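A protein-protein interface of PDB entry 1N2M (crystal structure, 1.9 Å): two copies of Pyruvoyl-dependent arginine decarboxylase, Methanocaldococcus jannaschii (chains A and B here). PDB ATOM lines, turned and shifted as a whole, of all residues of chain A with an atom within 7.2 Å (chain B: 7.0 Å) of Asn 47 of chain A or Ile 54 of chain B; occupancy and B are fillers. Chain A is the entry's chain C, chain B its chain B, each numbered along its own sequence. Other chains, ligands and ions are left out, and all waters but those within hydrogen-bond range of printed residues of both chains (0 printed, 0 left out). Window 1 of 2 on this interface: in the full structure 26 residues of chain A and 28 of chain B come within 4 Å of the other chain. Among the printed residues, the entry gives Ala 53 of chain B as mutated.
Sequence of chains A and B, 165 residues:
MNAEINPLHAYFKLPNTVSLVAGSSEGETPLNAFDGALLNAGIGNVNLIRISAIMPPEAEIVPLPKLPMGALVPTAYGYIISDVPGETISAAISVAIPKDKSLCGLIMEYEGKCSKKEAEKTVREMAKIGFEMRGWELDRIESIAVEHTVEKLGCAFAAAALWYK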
ATOM      1  N   ASP A  35     -27.826 -24.234 -10.883  1.00  0.00           N
ATOM      2  CA  ASP A  35     -27.107 -23.289 -10.030  1.00  0.00           C
ATOM      3  C   ASP A  35     -27.907 -21.992  -9.913  1.00  0.00           C
ATOM      4  O   ASP A  35     -28.112 -21.474  -8.812  1.00  0.00           O
ATOM      5  CB  ASP A  35     -25.722 -23.007 -10.630  1.00  0.00           C
ATOM      6  CG  ASP A  35     -24.858 -22.102  -9.749  1.00  0.00           C
ATOM      7  OD1 ASP A  35     -24.785 -22.325  -8.523  1.00  0.00           O
ATOM      8  OD2 ASP A  35     -24.218 -21.183 -10.300  1.00  0.00           O
ATOM      9  N   LEU A  38     -30.912 -22.381  -7.582  1.00  0.00           N
ATOM     10  CA  LEU A  38     -30.559 -22.407  -6.156  1.00  0.00           C
ATOM     11  C   LEU A  38     -30.415 -20.965  -5.666  1.00  0.00           C
ATOM     12  O   LEU A  38     -30.915 -20.603  -4.600  1.00  0.00           O
ATOM     13  CB  LEU A  38     -29.238 -23.154  -5.922  1.00  0.00           C
ATOM     14  CG  LEU A  38     -29.117 -24.620  -6.346  1.00  0.00           C
ATOM     15  CD1 LEU A  38     -27.865 -25.236  -5.737  1.00  0.00           C
ATOM     16  CD2 LEU A  38     -30.322 -25.377  -5.892  1.00  0.00           C
ATOM     17  N   ILE A  43     -30.669 -20.284  -1.847  1.00  0.00           N
ATOM     18  CA  ILE A  43     -29.793 -21.300  -1.290  1.00  0.00           C
ATOM     19  C   ILE A  43     -28.694 -21.654  -2.303  1.00  0.00           C
ATOM     20  O   ILE A  43     -28.224 -22.792  -2.364  1.00  0.00           O
ATOM     21  CB  ILE A  43     -30.652 -22.538  -0.888  1.00  0.00           C
ATOM     22  CG1 ILE A  43     -29.885 -23.458   0.056  1.00  0.00           C
ATOM     23  CG2 ILE A  43     -31.157 -23.274  -2.125  1.00  0.00           C
ATOM     24  CD1 ILE A  43     -30.747 -24.544   0.659  1.00  0.00           C
ATOM     25  N   GLY A  44     -28.253 -20.646  -3.057  1.00  0.00           N
ATOM     26  CA  GLY A  44     -27.231 -20.850  -4.076  1.00  0.00           C
ATOM     27  C   GLY A  44     -25.744 -20.922  -3.784  1.00  0.00           C
ATOM     28  O   GLY A  44     -24.965 -21.295  -4.671  1.00  0.00           O
ATOM     29  N   ASN A  45     -25.328 -20.577  -2.574  1.00  0.00           N
ATOM     30  CA  ASN A  45     -23.901 -20.611  -2.259  1.00  0.00           C
ATOM     31  C   ASN A  45     -23.553 -21.558  -1.123  1.00  0.00           C
ATOM     32  O   ASN A  45     -22.655 -21.295  -0.324  1.00  0.00           O
ATOM     33  CB  ASN A  45     -23.402 -19.194  -1.975  1.00  0.00           C
ATOM     34  CG  ASN A  45     -23.430 -18.318  -3.213  1.00  0.00           C
ATOM     35  OD1 ASN A  45     -23.050 -18.757  -4.302  1.00  0.00           O
ATOM     36  ND2 ASN A  45     -23.866 -17.073  -3.053  1.00  0.00           N
ATOM     37  N   VAL A  46     -24.268 -22.678  -1.072  1.00  0.00           N
ATOM     38  CA  VAL A  46     -24.045 -23.683  -0.046  1.00  0.00           C
ATOM     39  C   VAL A  46     -23.962 -25.062  -0.690  1.00  0.00           C
ATOM     40  O   VAL A  46     -24.356 -25.244  -1.841  1.00  0.00           O
ATOM     41  CB  VAL A  46     -25.192 -23.702   1.006  1.00  0.00           C
ATOM     42  CG1 VAL A  46     -25.353 -22.332   1.647  1.00  0.00           C
ATOM     43  CG2 VAL A  46     -26.502 -24.153   0.366  1.00  0.00           C
ATOM     44  N   ASN A  47     -23.421 -26.020   0.050  1.00  0.00           N
ATOM     45  CA  ASN A  47     -23.320 -27.389  -0.432  1.00  0.00           C
ATOM     46  C   ASN A  47     -24.587 -28.135  -0.030  1.00  0.00           C
ATOM     47  O   ASN A  47     -24.853 -28.320   1.158  1.00  0.00           O
ATOM     48  CB  ASN A  47     -22.099 -28.085   0.172  1.00  0.00           C
ATOM     49  CG  ASN A  47     -20.798 -27.651  -0.478  1.00  0.00           C
ATOM     50  OD1 ASN A  47     -20.583 -27.885  -1.662  1.00  0.00           O
ATOM     51  ND2 ASN A  47     -19.928 -27.013   0.295  1.00  0.00           N
ATOM     52  N   LEU A  48     -25.387 -28.527  -1.017  1.00  0.00           N
ATOM     53  CA  LEU A  48     -26.612 -29.262  -0.739  1.00  0.00           C
ATOM     54  C   LEU A  48     -26.339 -30.754  -0.639  1.00  0.00           C
ATOM     55  O   LEU A  48     -25.807 -31.359  -1.569  1.00  0.00           O
ATOM     56  CB  LEU A  48     -27.673 -29.034  -1.825  1.00  0.00           C
ATOM     57  CG  LEU A  48     -28.271 -27.641  -2.011  1.00  0.00           C
ATOM     58  CD1 LEU A  48     -29.460 -27.742  -2.948  1.00  0.00           C
ATOM     59  CD2 LEU A  48     -28.699 -27.069  -0.683  1.00  0.00           C
ATOM     60  N   ILE A  49     -26.662 -31.327   0.513  1.00  0.00           N
ATOM     61  CA  ILE A  49     -26.509 -32.758   0.721  1.00  0.00           C
ATOM     62  C   ILE A  49     -27.928 -33.293   0.613  1.00  0.00           C
ATOM     63  O   ILE A  49     -28.759 -33.049   1.486  1.00  0.00           O
ATOM     64  CB  ILE A  49     -25.965 -33.085   2.119  1.00  0.00           C
ATOM     65  CG1 ILE A  49     -24.576 -32.472   2.303  1.00  0.00           C
ATOM     66  CG2 ILE A  49     -25.908 -34.601   2.309  1.00  0.00           C
ATOM     67  CD1 ILE A  49     -24.034 -32.622   3.705  1.00  0.00           C
ATOM     68  N   ARG A  50     -28.221 -33.997  -0.470  1.00  0.00           N
ATOM     69  CA  ARG A  50     -29.567 -34.514  -0.652  1.00  0.00           C
ATOM     70  C   ARG A  50     -29.974 -35.577   0.370  1.00  0.00           C
ATOM     71  O   ARG A  50     -29.239 -36.533   0.625  1.00  0.00           O
ATOM     72  CB  ARG A  50     -29.756 -35.043  -2.070  1.00  0.00           C
ATOM     73  CG  ARG A  50     -31.218 -35.140  -2.469  1.00  0.00           C
ATOM     74  CD  ARG A  50     -31.371 -35.380  -3.954  1.00  0.00           C
ATOM     75  NE  ARG A  50     -32.753 -35.193  -4.389  1.00  0.00           N
ATOM     76  CZ  ARG A  50     -33.148 -35.261  -5.655  1.00  0.00           C
ATOM     77  NH1 ARG A  50     -32.265 -35.515  -6.616  1.00  0.00           N
ATOM     78  NH2 ARG A  50     -34.421 -35.057  -5.964  1.00  0.00           N
ATOM     79  N   PRO A  68     -24.180 -19.701   5.973  1.00  0.00           N
ATOM     80  CA  PRO A  68     -22.791 -19.334   5.675  1.00  0.00           C
ATOM     81  C   PRO A  68     -22.429 -19.999   4.352  1.00  0.00           C
ATOM     82  O   PRO A  68     -22.856 -21.125   4.096  1.00  0.00           O
ATOM     83  CB  PRO A  68     -22.012 -19.974   6.826  1.00  0.00           C
ATOM     84  CG  PRO A  68     -23.030 -20.091   7.928  1.00  0.00           C
ATOM     85  CD  PRO A  68     -24.253 -20.534   7.185  1.00  0.00           C
ATOM     86  N   MET A  69     -21.677 -19.305   3.503  1.00  0.00           N
ATOM     87  CA  MET A  69     -21.292 -19.873   2.218  1.00  0.00           C
ATOM     88  C   MET A  69     -20.509 -21.168   2.390  1.00  0.00           C
ATOM     89  O   MET A  69     -19.655 -21.276   3.276  1.00  0.00           O
ATOM     90  CB  MET A  69     -20.475 -18.870   1.403  1.00  0.00           C
ATOM     91  CG  MET A  69     -21.238 -17.620   1.016  1.00  0.00           C
ATOM     92  SD  MET A  69     -20.296 -16.632  -0.154  1.00  0.00           S
ATOM     93  CE  MET A  69     -21.397 -15.261  -0.412  1.00  0.00           C
ATOM     94  N   GLY A  70     -20.811 -22.150   1.542  1.00  0.00           N
ATOM     95  CA  GLY A  70     -20.135 -23.432   1.617  1.00  0.00           C
ATOM     96  C   GLY A  70     -20.709 -24.376   2.655  1.00  0.00           C
ATOM     97  O   GLY A  70     -20.250 -25.509   2.790  1.00  0.00           O
ATOM     98  N   ALA A  71     -21.721 -23.922   3.388  1.00  0.00           N
ATOM     99  CA  ALA A  71     -22.341 -24.750   4.414  1.00  0.00           C
ATOM    100  C   ALA A  71     -22.848 -26.069   3.837  1.00  0.00           C
ATOM    101  O   ALA A  71     -23.283 -26.126   2.686  1.00  0.00           O
ATOM    102  CB  ALA A  71     -23.499 -23.993   5.072  1.00  0.00           C
ATOM    103  N   LEU A  72     -22.719 -27.139   4.616  1.00  0.00           N
ATOM    104  CA  LEU A  72     -23.205 -28.454   4.203  1.00  0.00           C
ATOM    105  C   LEU A  72     -24.633 -28.520   4.729  1.00  0.00           C
ATOM    106  O   LEU A  72     -24.863 -28.712   5.927  1.00  0.00           O
ATOM    107  CB  LEU A  72     -22.337 -29.554   4.804  1.00  0.00           C
ATOM    108  CG  LEU A  72     -20.940 -29.621   4.178  1.00  0.00           C
ATOM    109  CD1 LEU A  72     -20.050 -30.545   4.981  1.00  0.00           C
ATOM    110  CD2 LEU A  72     -21.047 -30.097   2.740  1.00  0.00           C
ATOM    111  N   VAL A  73     -25.582 -28.331   3.820  1.00  0.00           N
ATOM    112  CA  VAL A  73     -26.997 -28.288   4.163  1.00  0.00           C
ATOM    113  C   VAL A  73     -27.802 -29.515   3.764  1.00  0.00           C
ATOM    114  O   VAL A  73     -27.995 -29.781   2.575  1.00  0.00           O
ATOM    115  CB  VAL A  73     -27.660 -27.033   3.531  1.00  0.00           C
ATOM    116  CG1 VAL A  73     -29.105 -26.890   3.999  1.00  0.00           C
ATOM    117  CG2 VAL A  73     -26.846 -25.774   3.868  1.00  0.00           C
ATOM    118  N   PRO A  74     -28.267 -30.292   4.757  1.00  0.00           N
ATOM    119  CA  PRO A  74     -29.064 -31.489   4.468  1.00  0.00           C
ATOM    120  C   PRO A  74     -30.329 -30.929   3.844  1.00  0.00           C
ATOM    121  O   PRO A  74     -31.040 -30.141   4.468  1.00  0.00           O
ATOM    122  CB  PRO A  74     -29.337 -32.063   5.856  1.00  0.00           C
ATOM    123  CG  PRO A  74     -28.197 -31.544   6.683  1.00  0.00           C
ATOM    124  CD  PRO A  74     -28.090 -30.123   6.208  1.00  0.00           C
ATOM    125  N   THR A  75     -30.592 -31.310   2.602  1.00  0.00           N
ATOM    126  CA  THR A  75     -31.731 -30.751   1.896  1.00  0.00           C
ATOM    127  C   THR A  75     -32.525 -31.750   1.083  1.00  0.00           C
ATOM    128  O   THR A  75     -31.966 -32.530   0.313  1.00  0.00           O
ATOM    129  CB  THR A  75     -31.255 -29.661   0.917  1.00  0.00           C
ATOM    130  OG1 THR A  75     -30.340 -28.783   1.581  1.00  0.00           O
ATOM    131  CG2 THR A  75     -32.428 -28.860   0.380  1.00  0.00           C
ATOM    132  N   LEU B  14     -16.885 -27.148   8.770  1.00  0.00           N
ATOM    133  CA  LEU B  14     -16.894 -27.167   7.306  1.00  0.00           C
ATOM    134  C   LEU B  14     -15.558 -27.592   6.697  1.00  0.00           C
ATOM    135  O   LEU B  14     -14.494 -27.256   7.213  1.00  0.00           O
ATOM    136  CB  LEU B  14     -17.257 -25.776   6.787  1.00  0.00           C
ATOM    137  CG  LEU B  14     -18.628 -25.498   6.168  1.00  0.00           C
ATOM    138  CD1 LEU B  14     -19.694 -26.440   6.687  1.00  0.00           C
ATOM    139  CD2 LEU B  14     -18.987 -24.037   6.408  1.00  0.00           C
ATOM    140  N   PRO B  15     -15.599 -28.360   5.593  1.00  0.00           N
ATOM    141  CA  PRO B  15     -14.356 -28.796   4.949  1.00  0.00           C
ATOM    142  C   PRO B  15     -13.590 -27.549   4.518  1.00  0.00           C
ATOM    143  O   PRO B  15     -14.201 -26.542   4.172  1.00  0.00           O
ATOM    144  CB  PRO B  15     -14.860 -29.575   3.735  1.00  0.00           C
ATOM    145  CG  PRO B  15     -16.181 -30.128   4.207  1.00  0.00           C
ATOM    146  CD  PRO B  15     -16.777 -28.949   4.930  1.00  0.00           C
ATOM    147  N   VAL B  18     -10.187 -28.670  -1.054  1.00  0.00           N
ATOM    148  CA  VAL B  18     -10.870 -29.230  -2.207  1.00  0.00           C
ATOM    149  C   VAL B  18      -9.781 -29.842  -3.071  1.00  0.00           C
ATOM    150  O   VAL B  18      -8.702 -29.269  -3.222  1.00  0.00           O
ATOM    151  CB  VAL B  18     -11.650 -28.152  -3.006  1.00  0.00           C
ATOM    152  CG1 VAL B  18     -12.223 -28.749  -4.292  1.00  0.00           C
ATOM    153  CG2 VAL B  18     -12.791 -27.595  -2.153  1.00  0.00           C
ATOM    154  N   ILE B  51     -22.490 -33.737  -3.620  1.00  0.00           N
ATOM    155  CA  ILE B  51     -22.932 -32.402  -3.242  1.00  0.00           C
ATOM    156  C   ILE B  51     -23.162 -31.527  -4.475  1.00  0.00           C
ATOM    157  O   ILE B  51     -22.645 -31.813  -5.560  1.00  0.00           O
ATOM    158  CB  ILE B  51     -21.920 -31.711  -2.297  1.00  0.00           C
ATOM    159  CG1 ILE B  51     -20.545 -31.626  -2.957  1.00  0.00           C
ATOM    160  CG2 ILE B  51     -21.853 -32.449  -0.966  1.00  0.00           C
ATOM    161  CD1 ILE B  51     -19.513 -30.878  -2.140  1.00  0.00           C
ATOM    162  N   SER B  52     -23.933 -30.456  -4.291  1.00  0.00           N
ATOM    163  CA  SER B  52     -24.256 -29.515  -5.361  1.00  0.00           C
ATOM    164  C   SER B  52     -23.036 -28.753  -5.885  1.00  0.00           C
ATOM    165  O   SER B  52     -23.106 -28.144  -6.960  1.00  0.00           O
ATOM    166  CB  SER B  52     -25.343 -28.541  -4.906  1.00  0.00           C
ATOM    167  OG  SER B  52     -24.969 -27.890  -3.704  1.00  0.00           O
ATOM    168  N   ALA B  53     -21.958 -28.736  -5.093  1.00  0.00           N
ATOM    169  CA  ALA B  53     -20.677 -28.114  -5.459  1.00  0.00           C
ATOM    170  C   ALA B  53     -20.363 -26.640  -5.147  1.00  0.00           C
ATOM    171  O   ALA B  53     -20.489 -25.769  -6.009  1.00  0.00           O
ATOM    172  CB  ALA B  53     -20.352 -28.414  -6.932  1.00  0.00           C
ATOM    173  N   ILE B  54     -19.859 -26.393  -3.940  1.00  0.00           N
ATOM    174  CA  ILE B  54     -19.462 -25.052  -3.504  1.00  0.00           C
ATOM    175  C   ILE B  54     -18.207 -25.159  -2.644  1.00  0.00           C
ATOM    176  O   ILE B  54     -18.193 -25.870  -1.641  1.00  0.00           O
ATOM    177  CB  ILE B  54     -20.565 -24.344  -2.665  1.00  0.00           C
ATOM    178  CG1 ILE B  54     -21.701 -23.868  -3.567  1.00  0.00           C
ATOM    179  CG2 ILE B  54     -19.978 -23.147  -1.906  1.00  0.00           C
ATOM    180  CD1 ILE B  54     -21.307 -22.753  -4.514  1.00  0.00           C
ATOM    181  N   MET B  55     -17.141 -24.487  -3.063  1.00  0.00           N
ATOM    182  CA  MET B  55     -15.903 -24.498  -2.295  1.00  0.00           C
ATOM    183  C   MET B  55     -16.048 -23.458  -1.191  1.00  0.00           C
ATOM    184  O   MET B  55     -16.209 -22.272  -1.472  1.00  0.00           O
ATOM    185  CB  MET B  55     -14.714 -24.158  -3.193  1.00  0.00           C
ATOM    186  CG  MET B  55     -13.419 -23.961  -2.429  1.00  0.00           C
ATOM    187  SD  MET B  55     -12.037 -23.663  -3.518  1.00  0.00           S
ATOM    188  CE  MET B  55     -10.749 -24.427  -2.607  1.00  0.00           C
ATOM    189  N   PRO B  56     -16.003 -23.889   0.081  1.00  0.00           N
ATOM    190  CA  PRO B  56     -16.139 -22.957   1.204  1.00  0.00           C
ATOM    191  C   PRO B  56     -15.122 -21.818   1.136  1.00  0.00           C
ATOM    192  O   PRO B  56     -14.002 -22.005   0.662  1.00  0.00           O
ATOM    193  CB  PRO B  56     -15.884 -23.852   2.419  1.00  0.00           C
ATOM    194  CG  PRO B  56     -16.370 -25.190   1.961  1.00  0.00           C
ATOM    195  CD  PRO B  56     -15.804 -25.265   0.568  1.00  0.00           C
ATOM    196  N   PRO B  57     -15.526 -20.607   1.549  1.00  0.00           N
ATOM    197  CA  PRO B  57     -14.626 -19.452   1.531  1.00  0.00           C
ATOM    198  C   PRO B  57     -13.355 -19.779   2.313  1.00  0.00           C
ATOM    199  O   PRO B  57     -13.407 -20.489   3.324  1.00  0.00           O
ATOM    200  CB  PRO B  57     -15.443 -18.380   2.246  1.00  0.00           C
ATOM    201  CG  PRO B  57     -16.841 -18.712   1.841  1.00  0.00           C
ATOM    202  CD  PRO B  57     -16.874 -20.216   1.998  1.00  0.00           C
ATOM    203  N   PRO B  74     -17.567 -35.293   1.187  1.00  0.00           N
ATOM    204  CA  PRO B  74     -18.520 -34.452   0.456  1.00  0.00           C
ATOM    205  C   PRO B  74     -17.857 -34.258  -0.900  1.00  0.00           C
ATOM    206  O   PRO B  74     -16.755 -33.715  -0.985  1.00  0.00           O
ATOM    207  CB  PRO B  74     -18.533 -33.154   1.273  1.00  0.00           C
ATOM    208  CG  PRO B  74     -18.144 -33.615   2.662  1.00  0.00           C
ATOM    209  CD  PRO B  74     -17.034 -34.580   2.360  1.00  0.00           C
ATOM    210  N   ALA B  76     -18.397 -33.278  -5.155  1.00  0.00           N
ATOM    211  CA  ALA B  76     -19.142 -32.829  -6.314  1.00  0.00           C
ATOM    212  C   ALA B  76     -18.486 -33.640  -7.420  1.00  0.00           C
ATOM    213  O   ALA B  76     -17.257 -33.699  -7.502  1.00  0.00           O
ATOM    214  CB  ALA B  76     -18.915 -31.361  -6.548  1.00  0.00           C
ATOM    215  N   VAL B  95     -13.202 -25.560 -10.697  1.00  0.00           N
ATOM    216  CA  VAL B  95     -13.471 -24.765  -9.516  1.00  0.00           C
ATOM    217  C   VAL B  95     -12.985 -23.351  -9.791  1.00  0.00           C
ATOM    218  O   VAL B  95     -11.815 -23.129 -10.116  1.00  0.00           O
ATOM    219  CB  VAL B  95     -12.802 -25.363  -8.255  1.00  0.00           C
ATOM    220  CG1 VAL B  95     -11.358 -25.709  -8.535  1.00  0.00           C
ATOM    221  CG2 VAL B  95     -12.915 -24.398  -7.081  1.00  0.00           C
ATOM    222  N   CYS B 104     -17.056 -17.708  -1.801  1.00  0.00           N
ATOM    223  CA  CYS B 104     -16.829 -19.127  -2.028  1.00  0.00           C
ATOM    224  C   CYS B 104     -16.404 -19.433  -3.464  1.00  0.00           C
ATOM    225  O   CYS B 104     -16.538 -18.598  -4.369  1.00  0.00           O
ATOM    226  CB  CYS B 104     -18.093 -19.912  -1.670  1.00  0.00           C
ATOM    227  SG  CYS B 104     -19.528 -19.446  -2.640  1.00  0.00           S
ATOM    228  N   GLY B 105     -15.817 -20.610  -3.647  1.00  0.00           N
ATOM    229  CA  GLY B 105     -15.411 -21.026  -4.972  1.00  0.00           C
ATOM    230  C   GLY B 105     -16.560 -21.811  -5.570  1.00  0.00           C
ATOM    231  O   GLY B 105     -17.303 -22.477  -4.845  1.00  0.00           O
ATOM    232  N   LEU B 106     -16.739 -21.706  -6.881  1.00  0.00           N
ATOM    233  CA  LEU B 106     -17.814 -22.425  -7.552  1.00  0.00           C
ATOM    234  C   LEU B 106     -17.275 -23.684  -8.214  1.00  0.00           C
ATOM    235  O   LEU B 106     -16.324 -23.631  -8.991  1.00  0.00           O
ATOM    236  CB  LEU B 106     -18.479 -21.540  -8.606  1.00  0.00           C
ATOM    237  CG  LEU B 106     -19.644 -22.194  -9.349  1.00  0.00           C
ATOM    238  CD1 LEU B 106     -20.813 -22.444  -8.406  1.00  0.00           C
ATOM    239  CD2 LEU B 106     -20.069 -21.307 -10.492  1.00  0.00           C
ATOM    240  N   ILE B 107     -17.878 -24.818  -7.882  1.00  0.00           N
ATOM    241  CA  ILE B 107     -17.468 -26.080  -8.446  1.00  0.00           C
ATOM    242  C   ILE B 107     -18.465 -26.509  -9.510  1.00  0.00           C
ATOM    243  O   ILE B 107     -19.676 -26.503  -9.290  1.00  0.00           O
ATOM    244  CB  ILE B 107     -17.327 -27.155  -7.350  1.00  0.00           C
ATOM    245  CG1 ILE B 107     -16.348 -26.670  -6.274  1.00  0.00           C
ATOM    246  CG2 ILE B 107     -16.826 -28.449  -7.950  1.00  0.00           C
ATOM    247  CD1 ILE B 107     -16.297 -27.552  -5.045  1.00  0.00           C
ATOM    248  N   ARG B 134     -23.153 -14.391 -10.624  1.00  0.00           N
ATOM    249  CA  ARG B 134     -23.042 -13.842  -9.278  1.00  0.00           C
ATOM    250  C   ARG B 134     -22.430 -12.445  -9.279  1.00  0.00           C
ATOM    251  O   ARG B 134     -22.627 -11.676  -8.336  1.00  0.00           O
ATOM    252  CB  ARG B 134     -22.201 -14.769  -8.395  1.00  0.00           C
ATOM    253  CG  ARG B 134     -22.863 -16.100  -8.072  1.00  0.00           C
ATOM    254  CD  ARG B 134     -21.898 -17.031  -7.370  1.00  0.00           C
ATOM    255  NE  ARG B 134     -22.553 -18.229  -6.846  1.00  0.00           N
ATOM    256  CZ  ARG B 134     -23.027 -19.220  -7.596  1.00  0.00           C
ATOM    257  NH1 ARG B 134     -22.924 -19.168  -8.919  1.00  0.00           N
ATOM    258  NH2 ARG B 134     -23.601 -20.267  -7.021  1.00  0.00           N
ATOM    259  N   TRP B 136     -19.195 -12.007  -9.490  1.00  0.00           N
ATOM    260  CA  TRP B 136     -17.969 -12.167  -8.717  1.00  0.00           C
ATOM    261  C   TRP B 136     -16.727 -12.122  -9.575  1.00  0.00           C
ATOM    262  O   TRP B 136     -16.666 -12.740 -10.638  1.00  0.00           O
ATOM    263  CB  TRP B 136     -17.970 -13.489  -7.959  1.00  0.00           C
ATOM    264  CG  TRP B 136     -18.990 -13.589  -6.885  1.00  0.00           C
ATOM    265  CD1 TRP B 136     -19.873 -12.629  -6.491  1.00  0.00           C
ATOM    266  CD2 TRP B 136     -19.220 -14.719  -6.045  1.00  0.00           C
ATOM    267  NE1 TRP B 136     -20.644 -13.092  -5.450  1.00  0.00           N
ATOM    268  CE2 TRP B 136     -20.261 -14.375  -5.157  1.00  0.00           C
ATOM    269  CE3 TRP B 136     -18.647 -15.992  -5.955  1.00  0.00           C
ATOM    270  CZ2 TRP B 136     -20.740 -15.259  -4.189  1.00  0.00           C
ATOM    271  CZ3 TRP B 136     -19.124 -16.868  -4.994  1.00  0.00           C
ATOM    272  CH2 TRP B 136     -20.160 -16.495  -4.123  1.00  0.00           C
ATOM    273  N   LEU B 162     -14.157 -32.550  -1.150  1.00  0.00           N
ATOM    274  CA  LEU B 162     -13.956 -31.626  -0.045  1.00  0.00           C
ATOM    275  C   LEU B 162     -13.457 -32.397   1.168  1.00  0.00           C
ATOM    276  O   LEU B 162     -14.014 -33.439   1.523  1.00  0.00           O
ATOM    277  CB  LEU B 162     -15.260 -30.904   0.322  1.00  0.00           C
ATOM    278  CG  LEU B 162     -15.762 -29.789  -0.598  1.00  0.00           C
ATOM    279  CD1 LEU B 162     -16.064 -30.340  -1.982  1.00  0.00           C
ATOM    280  CD2 LEU B 162     -17.006 -29.159   0.013  1.00  0.00           C
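Position printed for both chains: 74.
Of the printed residues of chain B, Asn 47 of chain A touches Ile 51 (3.2 Å), Ser 52 (3.7 Å), Ala 53 (3.7 Å), Ile 54 (2.8 Å) and Leu 162 (3.6 Å).
Pro 68 of chain A touches none of the printed residues of chain B.
Printed residues of chain A within 4 Å of Ser 52 of chain B: Val 46, Asn 47 and Leu 48.
Ile 54 of chain B touches five residues of chain A.
Pro 74 of chain B touches none of the printed residues of chain A.
Printed residues of chain A within 4 Å of Arg 134 of chain B: Asp 35 (2.8 Å), Gly 44 (2.9 Å) and Asn 45 (2.6 Å).
Printed residues of chain A within 4 Å of Leu 162 of chain B: Asn 47 (3.6 Å).
The nearest residue of chain B that does not touch Asn 47 of chain A is Pro 56 of chain B (4.3 Å).
The nearest printed residue of chain A that does not touch Pro 57 of chain B is Gly 70 of chain A (4.4 Å).
The backbone carbonyl oxygen (O) of Gly 44 of chain A is in hydrogen-bond range of the guanidinium group (NH2) of Arg 134 of chain B, 2.9 Å away.
The side-chain hydroxyl (OG) of Ser 52 of chain B lies within hydrogen-bond range of the backbone NH (N) of Leu 48 of chain A, 2.8 Å away.
The side-chain carboxylate (OD2) of Asp 35 of chain A is in salt-bridge range of the guanidinium group (NH1) of Arg 134 of chain B (2.8 Å).
The guanidinium group (NE) of Arg 134 of chain B lies within hydrogen-bond range of the side-chain amide oxygen (OD1) of Asn 45 of chain A, at 2.6 Å.
N of Cys 104 of chain B is in hydrogen-bond range of SD of Met 69 of chain A, 3.8 Å away.
N of Ile 54 of chain B sits at hydrogen-bond distance from OD1 of Asn 47 of chain A, at 2.8 Å.
The side-chain hydroxyl (OG) of Ser 52 of chain B is in hydrogen-bond range of the backbone carbonyl oxygen (O) of Val 46 of chain A, at 3.3 Å.
Among the printed residues, merely in contact across the chains: Asp 35 of chain A with Leu 106 of chain B (3.98 Å), Gly 44 of chain A with Ile 54 of chain B (3.9 Å), Asn 45 of chain A with Ile 54 of chain B (3.6 Å), Asn 45 of chain A with Cys 104 of chain B (3.9 Å), Asn 45 of chain A with Trp 136 of chain B (3.7 Å), Val 46 of chain A with Ile 54 of chain B (3.5 Å), Asn 47 of chain A with Ile 51 of chain B (3.2 Å), Asn 47 of chain A with Ser 52 of chain B (3.7 Å), Asn 47 of chain A with Ala 53 of chain B (3.7 Å), Asn 47 of chain A with Leu 162 of chain B (3.6 Å), Leu 48 of chain A with Ile 51 of chain B (3.5 Å), Met 69 of chain A with Pro 57 of chain B (3.2 Å), Met 69 of chain A with Trp 136 of chain B (3.8 Å), Gly 70 of chain A with Leu 14 of chain B (3.7 Å), Gly 70 of chain A with Ile 54 of chain B (3.5 Å), Gly 70 of chain A with Pro 56 of chain B (3.98 Å), Ala 71 of chain A with Leu 14 of chain B (3.9 Å), Leu 72 of chain A with Leu 14 of chain B (3.7 Å) and Leu 72 of chain A with Pro 15 of chain B (3.6 Å).
Of the 18 printed residues of chain A, 10 touch a printed residue of chain B.
Hydrophobic or aromatic side chains of chain A within 4 Å of the printed part of chain B: Leu 48, Met 69 and Leu 72.
Of the 20 printed residues of chain B, 13 touch a printed residue of chain A.
Hydrophobic or aromatic side chains of chain B that line the printed part of chain A: Leu 14, Pro 15, Ile 51, Ile 54, Pro 56, Pro 57, Leu 106, Trp 136 and Leu 162.
O of Gly 70 of chain A lies within hydrogen-bond range of ND2 of Asn 47 of chain A (2.9 Å).
N of Gly 70 of chain A is in hydrogen-bond range of O of Asn 45 of chain A, 2.8 Å away.
N of Ile 107 of chain B sits at hydrogen-bond distance from O of Ala 53 of chain B (3.4 Å).
The backbone NH of Val 73 of chain A sits at hydrogen-bond distance from the backbone carbonyl oxygen of Asn 47 of chain A, at 2.8 Å.
The backbone NH (N) of Asn 47 of chain A lies within hydrogen-bond range of the backbone carbonyl oxygen (O) of Ala 71 of chain A, 2.6 Å away.
N of Leu 162 of chain B sits at hydrogen-bond distance from O of Pro 74 of chain B (2.9 Å).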
